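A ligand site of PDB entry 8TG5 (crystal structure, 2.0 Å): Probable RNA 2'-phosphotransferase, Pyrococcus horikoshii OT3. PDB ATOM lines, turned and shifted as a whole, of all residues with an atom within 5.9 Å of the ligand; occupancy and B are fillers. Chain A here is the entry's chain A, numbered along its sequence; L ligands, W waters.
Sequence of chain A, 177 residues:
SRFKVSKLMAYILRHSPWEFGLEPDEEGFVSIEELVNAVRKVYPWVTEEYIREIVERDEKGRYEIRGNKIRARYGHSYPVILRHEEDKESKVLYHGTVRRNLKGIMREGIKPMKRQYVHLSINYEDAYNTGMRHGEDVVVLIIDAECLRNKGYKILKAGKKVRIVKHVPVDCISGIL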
ATOM      1  N   ARG A   2      -7.485  -3.885   4.878  1.00  0.00           N
ATOM      2  CA  ARG A   2      -8.340  -4.941   5.411  1.00  0.00           C
ATOM      3  C   ARG A   2      -9.471  -5.249   4.452  1.00  0.00           C
ATOM      4  O   ARG A   2      -9.878  -6.404   4.347  1.00  0.00           O
ATOM      5  CB  ARG A   2      -8.891  -4.556   6.791  1.00  0.00           C
ATOM      6  CG  ARG A   2      -7.849  -4.796   7.922  1.00  0.00           C
ATOM      7  CD  ARG A   2      -8.417  -4.503   9.304  1.00  0.00           C
ATOM      8  NE  ARG A   2      -9.046  -3.190   9.365  1.00  0.00           N
ATOM      9  CZ  ARG A   2     -10.355  -2.986   9.492  1.00  0.00           C
ATOM     10  NH1 ARG A   2     -11.206  -3.990   9.610  1.00  0.00           N
ATOM     11  NH2 ARG A   2     -10.814  -1.729   9.505  1.00  0.00           N
ATOM     12  N   PHE A   3      -9.987  -4.245   3.737  1.00  0.00           N
ATOM     13  CA  PHE A   3     -11.085  -4.513   2.811  1.00  0.00           C
ATOM     14  C   PHE A   3     -10.657  -5.482   1.707  1.00  0.00           C
ATOM     15  O   PHE A   3     -11.326  -6.490   1.438  1.00  0.00           O
ATOM     16  CB  PHE A   3     -11.634  -3.221   2.195  1.00  0.00           C
ATOM     17  CG  PHE A   3     -12.665  -3.470   1.129  1.00  0.00           C
ATOM     18  CD1 PHE A   3     -13.957  -3.839   1.473  1.00  0.00           C
ATOM     19  CD2 PHE A   3     -12.343  -3.358  -0.223  1.00  0.00           C
ATOM     20  CE1 PHE A   3     -14.926  -4.083   0.483  1.00  0.00           C
ATOM     21  CE2 PHE A   3     -13.290  -3.603  -1.210  1.00  0.00           C
ATOM     22  CZ  PHE A   3     -14.586  -3.967  -0.860  1.00  0.00           C
ATOM     23  N   SER A   6      -9.943  -8.996   3.253  1.00  0.00           N
ATOM     24  CA  SER A   6     -11.210  -9.615   3.660  1.00  0.00           C
ATOM     25  C   SER A   6     -12.023 -10.042   2.445  1.00  0.00           C
ATOM     26  O   SER A   6     -12.663 -11.099   2.456  1.00  0.00           O
ATOM     27  CB  SER A   6     -12.039  -8.621   4.492  1.00  0.00           C
ATOM     28  OG  SER A   6     -13.190  -9.232   5.050  1.00  0.00           O
ATOM     29  N   LYS A   7     -12.036  -9.220   1.400  1.00  0.00           N
ATOM     30  CA  LYS A   7     -12.793  -9.601   0.214  1.00  0.00           C
ATOM     31  C   LYS A   7     -12.267 -10.914  -0.346  1.00  0.00           C
ATOM     32  O   LYS A   7     -13.048 -11.798  -0.708  1.00  0.00           O
ATOM     33  CB  LYS A   7     -12.774  -8.499  -0.839  1.00  0.00           C
ATOM     34  CG  LYS A   7     -13.836  -7.417  -0.641  1.00  0.00           C
ATOM     35  CD  LYS A   7     -15.203  -7.829  -1.223  1.00  0.00           C
ATOM     36  CE  LYS A   7     -15.207  -7.704  -2.719  1.00  0.00           C
ATOM     37  NZ  LYS A   7     -16.484  -8.235  -3.280  1.00  0.00           N
ATOM     38  N   LEU A   8     -10.940 -11.083  -0.362  1.00  0.00           N
ATOM     39  CA  LEU A   8     -10.355 -12.338  -0.858  1.00  0.00           C
ATOM     40  C   LEU A   8     -10.606 -13.498   0.092  1.00  0.00           C
ATOM     41  O   LEU A   8     -10.837 -14.626  -0.355  1.00  0.00           O
ATOM     42  CB  LEU A   8      -8.860 -12.166  -1.107  1.00  0.00           C
ATOM     43  CG  LEU A   8      -8.046 -13.414  -1.520  1.00  0.00           C
ATOM     44  CD1 LEU A   8      -8.552 -14.041  -2.825  1.00  0.00           C
ATOM     45  CD2 LEU A   8      -6.565 -13.063  -1.647  1.00  0.00           C
ATOM     46  N   ALA A  10     -13.224 -13.917   1.988  1.00  0.00           N
ATOM     47  CA  ALA A  10     -14.607 -14.343   1.785  1.00  0.00           C
ATOM     48  C   ALA A  10     -14.726 -15.206   0.537  1.00  0.00           C
ATOM     49  O   ALA A  10     -15.405 -16.244   0.551  1.00  0.00           O
ATOM     50  CB  ALA A  10     -15.528 -13.133   1.697  1.00  0.00           C
ATOM     51  N   TYR A  11     -14.061 -14.795  -0.542  1.00  0.00           N
ATOM     52  CA  TYR A  11     -14.119 -15.549  -1.792  1.00  0.00           C
ATOM     53  C   TYR A  11     -13.562 -16.946  -1.610  1.00  0.00           C
ATOM     54  O   TYR A  11     -14.164 -17.939  -2.043  1.00  0.00           O
ATOM     55  CB  TYR A  11     -13.370 -14.800  -2.889  1.00  0.00           C
ATOM     56  CG  TYR A  11     -13.233 -15.566  -4.188  1.00  0.00           C
ATOM     57  CD1 TYR A  11     -14.260 -15.582  -5.119  1.00  0.00           C
ATOM     58  CD2 TYR A  11     -12.073 -16.270  -4.468  1.00  0.00           C
ATOM     59  CE1 TYR A  11     -14.132 -16.276  -6.310  1.00  0.00           C
ATOM     60  CE2 TYR A  11     -11.941 -16.969  -5.667  1.00  0.00           C
ATOM     61  CZ  TYR A  11     -12.973 -16.968  -6.572  1.00  0.00           C
ATOM     62  OH  TYR A  11     -12.829 -17.666  -7.749  1.00  0.00           O
ATOM     63  N   ARG A  14     -15.957 -18.993   1.088  1.00  0.00           N
ATOM     64  CA  ARG A  14     -17.329 -19.242   0.661  1.00  0.00           C
ATOM     65  C   ARG A  14     -17.413 -19.930  -0.697  1.00  0.00           C
ATOM     66  O   ARG A  14     -18.389 -20.654  -0.952  1.00  0.00           O
ATOM     67  CB  ARG A  14     -18.127 -17.935   0.564  1.00  0.00           C
ATOM     68  CG  ARG A  14     -18.523 -17.269   1.873  1.00  0.00           C
ATOM     69  CD  ARG A  14     -18.988 -15.869   1.551  1.00  0.00           C
ATOM     70  NE  ARG A  14     -19.262 -15.031   2.710  1.00  0.00           N
ATOM     71  CZ  ARG A  14     -19.456 -13.719   2.626  1.00  0.00           C
ATOM     72  NH1 ARG A  14     -19.539 -13.103   1.453  1.00  0.00           N
ATOM     73  NH2 ARG A  14     -19.577 -13.000   3.747  1.00  0.00           N
ATOM     74  N   HIS A  15     -16.448 -19.712  -1.581  1.00  0.00           N
ATOM     75  CA  HIS A  15     -16.778 -19.992  -2.979  1.00  0.00           C
ATOM     76  C   HIS A  15     -15.716 -20.788  -3.715  1.00  0.00           C
ATOM     77  O   HIS A  15     -16.066 -21.608  -4.581  1.00  0.00           O
ATOM     78  CB  HIS A  15     -17.021 -18.675  -3.743  1.00  0.00           C
ATOM     79  CG  HIS A  15     -18.169 -17.853  -3.208  1.00  0.00           C
ATOM     80  ND1 HIS A  15     -19.443 -18.362  -3.055  1.00  0.00           N
ATOM     81  CD2 HIS A  15     -18.225 -16.560  -2.813  1.00  0.00           C
ATOM     82  CE1 HIS A  15     -20.228 -17.410  -2.571  1.00  0.00           C
ATOM     83  NE2 HIS A  15     -19.510 -16.312  -2.410  1.00  0.00           N
ATOM     84  N   ASP A  58     -14.091  -7.597  12.175  1.00  0.00           N
ATOM     85  CA  ASP A  58     -15.053  -7.576  11.076  1.00  0.00           C
ATOM     86  C   ASP A  58     -16.415  -7.060  11.538  1.00  0.00           C
ATOM     87  O   ASP A  58     -16.957  -7.513  12.544  1.00  0.00           O
ATOM     88  CB  ASP A  58     -15.182  -8.976  10.476  1.00  0.00           C
ATOM     89  CG  ASP A  58     -16.125  -8.993   9.306  1.00  0.00           C
ATOM     90  OD1 ASP A  58     -17.340  -9.075   9.552  1.00  0.00           O
ATOM     91  OD2 ASP A  58     -15.648  -8.904   8.154  1.00  0.00           O
ATOM     92  N   GLU A  59     -16.960  -6.102  10.783  1.00  0.00           N
ATOM     93  CA  GLU A  59     -18.178  -5.406  11.186  1.00  0.00           C
ATOM     94  C   GLU A  59     -19.399  -6.335  11.225  1.00  0.00           C
ATOM     95  O   GLU A  59     -20.293  -6.155  12.052  1.00  0.00           O
ATOM     96  CB  GLU A  59     -18.453  -4.227  10.241  1.00  0.00           C
ATOM     97  CG  GLU A  59     -17.422  -3.084  10.301  1.00  0.00           C
ATOM     98  CD  GLU A  59     -16.018  -3.501   9.833  1.00  0.00           C
ATOM     99  OE1 GLU A  59     -15.018  -2.891  10.286  1.00  0.00           O
ATOM    100  OE2 GLU A  59     -15.901  -4.448   9.006  1.00  0.00           O
ATOM    101  N   LYS A  60     -19.464  -7.316  10.323  1.00  0.00           N
ATOM    102  CA  LYS A  60     -20.638  -8.184  10.247  1.00  0.00           C
ATOM    103  C   LYS A  60     -20.452  -9.497  10.986  1.00  0.00           C
ATOM    104  O   LYS A  60     -21.394 -10.294  11.031  1.00  0.00           O
ATOM    105  CB  LYS A  60     -20.982  -8.467   8.786  1.00  0.00           C
ATOM    106  CG  LYS A  60     -21.435  -7.241   8.001  1.00  0.00           C
ATOM    107  CD  LYS A  60     -21.572  -7.545   6.518  1.00  0.00           C
ATOM    108  CE  LYS A  60     -22.922  -8.133   6.149  1.00  0.00           C
ATOM    109  NZ  LYS A  60     -23.295  -7.743   4.753  1.00  0.00           N
ATOM    110  N   ARG A  62     -18.290 -11.794   9.900  1.00  0.00           N
ATOM    111  CA  ARG A  62     -18.302 -12.695   8.748  1.00  0.00           C
ATOM    112  C   ARG A  62     -17.581 -14.006   9.024  1.00  0.00           C
ATOM    113  O   ARG A  62     -17.838 -14.993   8.328  1.00  0.00           O
ATOM    114  CB  ARG A  62     -17.640 -12.042   7.541  1.00  0.00           C
ATOM    115  CG  ARG A  62     -18.376 -10.830   6.966  1.00  0.00           C
ATOM    116  CD  ARG A  62     -17.742 -10.412   5.652  1.00  0.00           C
ATOM    117  NE  ARG A  62     -18.439  -9.295   5.032  1.00  0.00           N
ATOM    118  CZ  ARG A  62     -18.253  -8.022   5.358  1.00  0.00           C
ATOM    119  NH1 ARG A  62     -17.383  -7.673   6.303  1.00  0.00           N
ATOM    120  NH2 ARG A  62     -18.910  -7.081   4.699  1.00  0.00           N
ATOM    121  N   TYR A  63     -16.653 -14.017   9.983  1.00  0.00           N
ATOM    122  CA  TYR A  63     -15.688 -15.106  10.119  1.00  0.00           C
ATOM    123  C   TYR A  63     -15.730 -15.670  11.525  1.00  0.00           C
ATOM    124  O   TYR A  63     -16.183 -15.026  12.478  1.00  0.00           O
ATOM    125  CB  TYR A  63     -14.257 -14.645   9.781  1.00  0.00           C
ATOM    126  CG  TYR A  63     -14.166 -13.931   8.449  1.00  0.00           C
ATOM    127  CD1 TYR A  63     -14.324 -14.637   7.268  1.00  0.00           C
ATOM    128  CD2 TYR A  63     -13.950 -12.560   8.382  1.00  0.00           C
ATOM    129  CE1 TYR A  63     -14.265 -13.988   6.048  1.00  0.00           C
ATOM    130  CE2 TYR A  63     -13.881 -11.901   7.162  1.00  0.00           C
ATOM    131  CZ  TYR A  63     -14.056 -12.628   6.000  1.00  0.00           C
ATOM    132  OH  TYR A  63     -13.990 -11.998   4.772  1.00  0.00           O
ATOM    133  N   TYR A  74     -21.294 -17.736   6.944  1.00  0.00           N
ATOM    134  CA  TYR A  74     -22.486 -17.746   6.114  1.00  0.00           C
ATOM    135  C   TYR A  74     -22.070 -17.475   4.675  1.00  0.00           C
ATOM    136  O   TYR A  74     -20.938 -17.067   4.411  1.00  0.00           O
ATOM    137  CB  TYR A  74     -23.523 -16.700   6.594  1.00  0.00           C
ATOM    138  CG  TYR A  74     -23.055 -15.243   6.511  1.00  0.00           C
ATOM    139  CD1 TYR A  74     -23.090 -14.538   5.302  1.00  0.00           C
ATOM    140  CD2 TYR A  74     -22.582 -14.580   7.642  1.00  0.00           C
ATOM    141  CE1 TYR A  74     -22.667 -13.217   5.222  1.00  0.00           C
ATOM    142  CE2 TYR A  74     -22.154 -13.252   7.575  1.00  0.00           C
ATOM    143  CZ  TYR A  74     -22.198 -12.579   6.370  1.00  0.00           C
ATOM    144  OH  TYR A  74     -21.761 -11.250   6.307  1.00  0.00           O
ATOM    145  N   GLY A  75     -23.007 -17.704   3.752  1.00  0.00           N
ATOM    146  CA  GLY A  75     -22.815 -17.289   2.372  1.00  0.00           C
ATOM    147  C   GLY A  75     -22.120 -18.285   1.470  1.00  0.00           C
ATOM    148  O   GLY A  75     -21.831 -17.935   0.326  1.00  0.00           O
ATOM    149  N   ARG A 133     -29.503  -6.624  -4.039  1.00  0.00           N
ATOM    150  CA  ARG A 133     -28.651  -7.524  -4.814  1.00  0.00           C
ATOM    151  C   ARG A 133     -29.387  -8.118  -6.010  1.00  0.00           C
ATOM    152  O   ARG A 133     -28.769  -8.353  -7.054  1.00  0.00           O
ATOM    153  CB  ARG A 133     -28.121  -8.664  -3.919  1.00  0.00           C
ATOM    154  CG  ARG A 133     -26.723  -8.456  -3.347  1.00  0.00           C
ATOM    155  CD  ARG A 133     -26.594  -9.074  -1.947  1.00  0.00           C
ATOM    156  NE  ARG A 133     -25.463  -8.544  -1.183  1.00  0.00           N
ATOM    157  CZ  ARG A 133     -25.244  -8.790   0.106  1.00  0.00           C
ATOM    158  NH1 ARG A 133     -26.073  -9.539   0.817  1.00  0.00           N
ATOM    159  NH2 ARG A 133     -24.174  -8.267   0.698  1.00  0.00           N
HETATM  160  C1  LIG L   1     -18.391 -13.256  -3.198  1.00  0.00           C
HETATM  161  C2  LIG L   1     -20.683 -10.090  -1.095  1.00  0.00           C
HETATM  162  C3  LIG L   1     -19.808  -9.468  -2.172  1.00  0.00           C
HETATM  163  C4  LIG L   1     -20.489  -8.318  -2.904  1.00  0.00           C
HETATM  164  C5  LIG L   1     -19.815  -4.323  -1.905  1.00  0.00           C
HETATM  165  C6  LIG L   1     -16.006 -10.257  -8.044  1.00  0.00           C
HETATM  166  C7  LIG L   1     -18.163 -10.744  -7.304  1.00  0.00           C
HETATM  167  C8  LIG L   1     -16.379 -11.478  -6.006  1.00  0.00           C
HETATM  168  C9  LIG L   1     -15.489 -10.933  -6.903  1.00  0.00           C
HETATM  169  C10 LIG L   1     -14.349 -11.868  -5.285  1.00  0.00           C
HETATM  170  C11 LIG L   1     -16.174 -12.759  -3.837  1.00  0.00           C
HETATM  171  C12 LIG L   1     -19.567 -12.518  -3.877  1.00  0.00           C
HETATM  172  C13 LIG L   1     -18.418  -3.910  -2.341  1.00  0.00           C
HETATM  173  C14 LIG L   1     -18.733  -2.853  -3.389  1.00  0.00           C
HETATM  174  C15 LIG L   1     -17.284  -1.392  -4.788  1.00  0.00           C
HETATM  175  C16 LIG L   1     -15.904  -0.527  -3.348  1.00  0.00           C
HETATM  176  C17 LIG L   1     -14.899   0.168  -2.618  1.00  0.00           C
HETATM  177  C18 LIG L   1     -15.667  -0.823  -0.665  1.00  0.00           C
HETATM  178  C19 LIG L   1     -16.775  -1.369  -2.677  1.00  0.00           C
HETATM  179  C20 LIG L   1     -20.658  -3.057  -2.056  1.00  0.00           C
HETATM  180  C21 LIG L   1     -20.898  -2.481  -0.665  1.00  0.00           C
HETATM  181  C22 LIG L   1     -18.710  -9.260  -0.108  1.00  0.00           C
HETATM  182  C23 LIG L   1     -18.453  -7.009   0.676  1.00  0.00           C
HETATM  183  C24 LIG L   1     -16.845  -7.317   2.105  1.00  0.00           C
HETATM  184  C25 LIG L   1     -15.809  -7.326   3.074  1.00  0.00           C
HETATM  185  C26 LIG L   1     -15.543  -9.621   2.778  1.00  0.00           C
HETATM  186  C27 LIG L   1     -17.160  -8.537   1.519  1.00  0.00           C
HETATM  187  C28 LIG L   1     -20.219  -9.403   0.181  1.00  0.00           C
HETATM  188  C29 LIG L   1     -17.704 -12.411  -2.109  1.00  0.00           C
HETATM  189  C30 LIG L   1     -16.667 -11.660  -2.900  1.00  0.00           C
HETATM  190  N1  LIG L   1     -15.119  -9.666  -9.020  1.00  0.00           N
HETATM  191  N2  LIG L   1     -17.329 -10.201  -8.179  1.00  0.00           N
HETATM  192  N3  LIG L   1     -17.705 -11.376  -6.219  1.00  0.00           N
HETATM  193  N4  LIG L   1     -14.238 -11.194  -6.436  1.00  0.00           N
HETATM  194  N5  LIG L   1     -15.622 -12.062  -5.020  1.00  0.00           N
HETATM  195  N6  LIG L   1     -17.618  -1.897  -3.612  1.00  0.00           N
HETATM  196  N7  LIG L   1     -16.249  -0.559  -4.647  1.00  0.00           N
HETATM  197  N8  LIG L   1     -13.967   1.070  -3.295  1.00  0.00           N
HETATM  198  N9  LIG L   1     -14.815  -0.006  -1.287  1.00  0.00           N
HETATM  199  N10 LIG L   1     -16.621  -1.491  -1.326  1.00  0.00           N
HETATM  200  N11 LIG L   1     -18.150  -8.310   0.653  1.00  0.00           N
HETATM  201  N12 LIG L   1     -17.671  -6.403   1.570  1.00  0.00           N
HETATM  202  N13 LIG L   1     -15.430  -6.093   3.732  1.00  0.00           N
HETATM  203  N14 LIG L   1     -15.198  -8.461   3.372  1.00  0.00           N
HETATM  204  N15 LIG L   1     -16.500  -9.637   1.864  1.00  0.00           N
HETATM  205  O1  LIG L   1     -17.339 -13.541  -4.167  1.00  0.00           O
HETATM  206  O2  LIG L   1     -20.859 -12.850  -3.295  1.00  0.00           O
HETATM  207  O3  LIG L   1     -20.591 -14.019  -1.017  1.00  0.00           O
HETATM  208  O4  LIG L   1     -22.579 -12.544  -1.306  1.00  0.00           O
HETATM  209  O5  LIG L   1     -20.293 -11.460  -0.928  1.00  0.00           O
HETATM  210  O6  LIG L   1     -21.365  -7.697  -1.934  1.00  0.00           O
HETATM  211  O7  LIG L   1     -22.088  -5.599  -0.758  1.00  0.00           O
HETATM  212  O8  LIG L   1     -22.892  -6.021  -3.063  1.00  0.00           O
HETATM  213  O9  LIG L   1     -20.406  -5.341  -2.760  1.00  0.00           O
HETATM  214  O10 LIG L   1     -17.723  -5.063  -2.913  1.00  0.00           O
HETATM  215  O11 LIG L   1     -19.895  -2.141  -2.877  1.00  0.00           O
HETATM  216  O12 LIG L   1     -20.451  -3.420   0.280  1.00  0.00           O
HETATM  217  O13 LIG L   1     -18.624  -8.933  -1.517  1.00  0.00           O
HETATM  218  O14 LIG L   1     -20.420 -10.331   1.311  1.00  0.00           O
HETATM  219  O15 LIG L   1     -20.704  -8.265   2.775  1.00  0.00           O
HETATM  220  O16 LIG L   1     -22.586  -9.843   2.560  1.00  0.00           O
HETATM  221  O17 LIG L   1     -20.620 -10.510   3.853  1.00  0.00           O
HETATM  222  O18 LIG L   1     -17.014 -13.255  -1.166  1.00  0.00           O
HETATM  223  O19 LIG L   1     -15.602 -11.224  -2.036  1.00  0.00           O
HETATM  224  P1  LIG L   1     -21.109 -12.728  -1.626  1.00  0.00           P
HETATM  225  P2  LIG L   1     -21.738  -6.123  -2.118  1.00  0.00           P
HETATM  226  P3  LIG L   1     -21.080  -9.705   2.665  1.00  0.00           P
HETATM  227  O   HOH W   1     -25.021 -12.319   2.782  1.00  0.00           O
HETATM  228  O   HOH W   2     -21.380  -5.982   1.714  1.00  0.00           O
HETATM  229  O   HOH W   3     -25.113 -12.720  -2.926  1.00  0.00           O
HETATM  230  O   HOH W   4     -13.646  -5.520   5.899  1.00  0.00           O
HETATM  231  O   HOH W   5     -15.838   3.246  -3.573  1.00  0.00           O
HETATM  232  O   HOH W   6     -16.836  -3.578   3.465  1.00  0.00           O
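NE of Arg 14 sits at hydrogen-bond distance from O of Tyr 74 (3.1 Å). The side-chain hydroxyl (OH) of Tyr 63 is in hydrogen-bond range of the backbone carbonyl oxygen (O) of Ser 6 (2.8 Å). The guanidinium group of Arg 62 is in salt-bridge range of the side-chain carboxylate of Asp 58. The backbone NH of Lys 60 is in hydrogen-bond range of the side-chain carboxylate of Asp 58, at 2.9 Å. The side-chain hydroxyl (OH) of Tyr 63 lies within hydrogen-bond range of the backbone NH (N) of Ala 10 (3.5 Å).
Residues that only touch the ligand: Ala 10, Phe 3 and Tyr 63. Hydrophobic or aromatic side chains that line the ligand: Phe 3, Ala 10, Tyr 11, His 15 and Tyr 74. Of the 17 residues printed, 12 come within 4 Å of the ligand.
An oxygen (O17) of the ligand lies within salt-bridge range of the guanidinium group (NH2) of Arg 14 (2.7 Å). The side-chain hydroxyl of Ser 6 lies within hydrogen-bond range of a nitrogen (N14) of the ligand, 2.7 Å away. The guanidinium group (NE) of Arg 62 is in salt-bridge range of an oxygen (O17) of the ligand. O17 of the ligand is in hydrogen-bond range of OH of Tyr 74. An oxygen (O19) of the ligand is in hydrogen-bond range of the backbone carbonyl oxygen of Lys 7 (2.9 Å). NZ of Lys 7 is in hydrogen-bond range of O13 of the ligand (2.9 Å). A ring nitrogen (NE2) of His 15 sits at hydrogen-bond distance from an oxygen (O3) of the ligand. NH2 of Arg 133 is in salt-bridge range of O16 of the ligand (2.9 Å). NZ of Lys 60 lies within salt-bridge range of O16 of the ligand (3.1 Å). The backbone NH (N) of Tyr 11 is in hydrogen-bond range of an oxygen (O18) of the ligand (3.4 Å).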
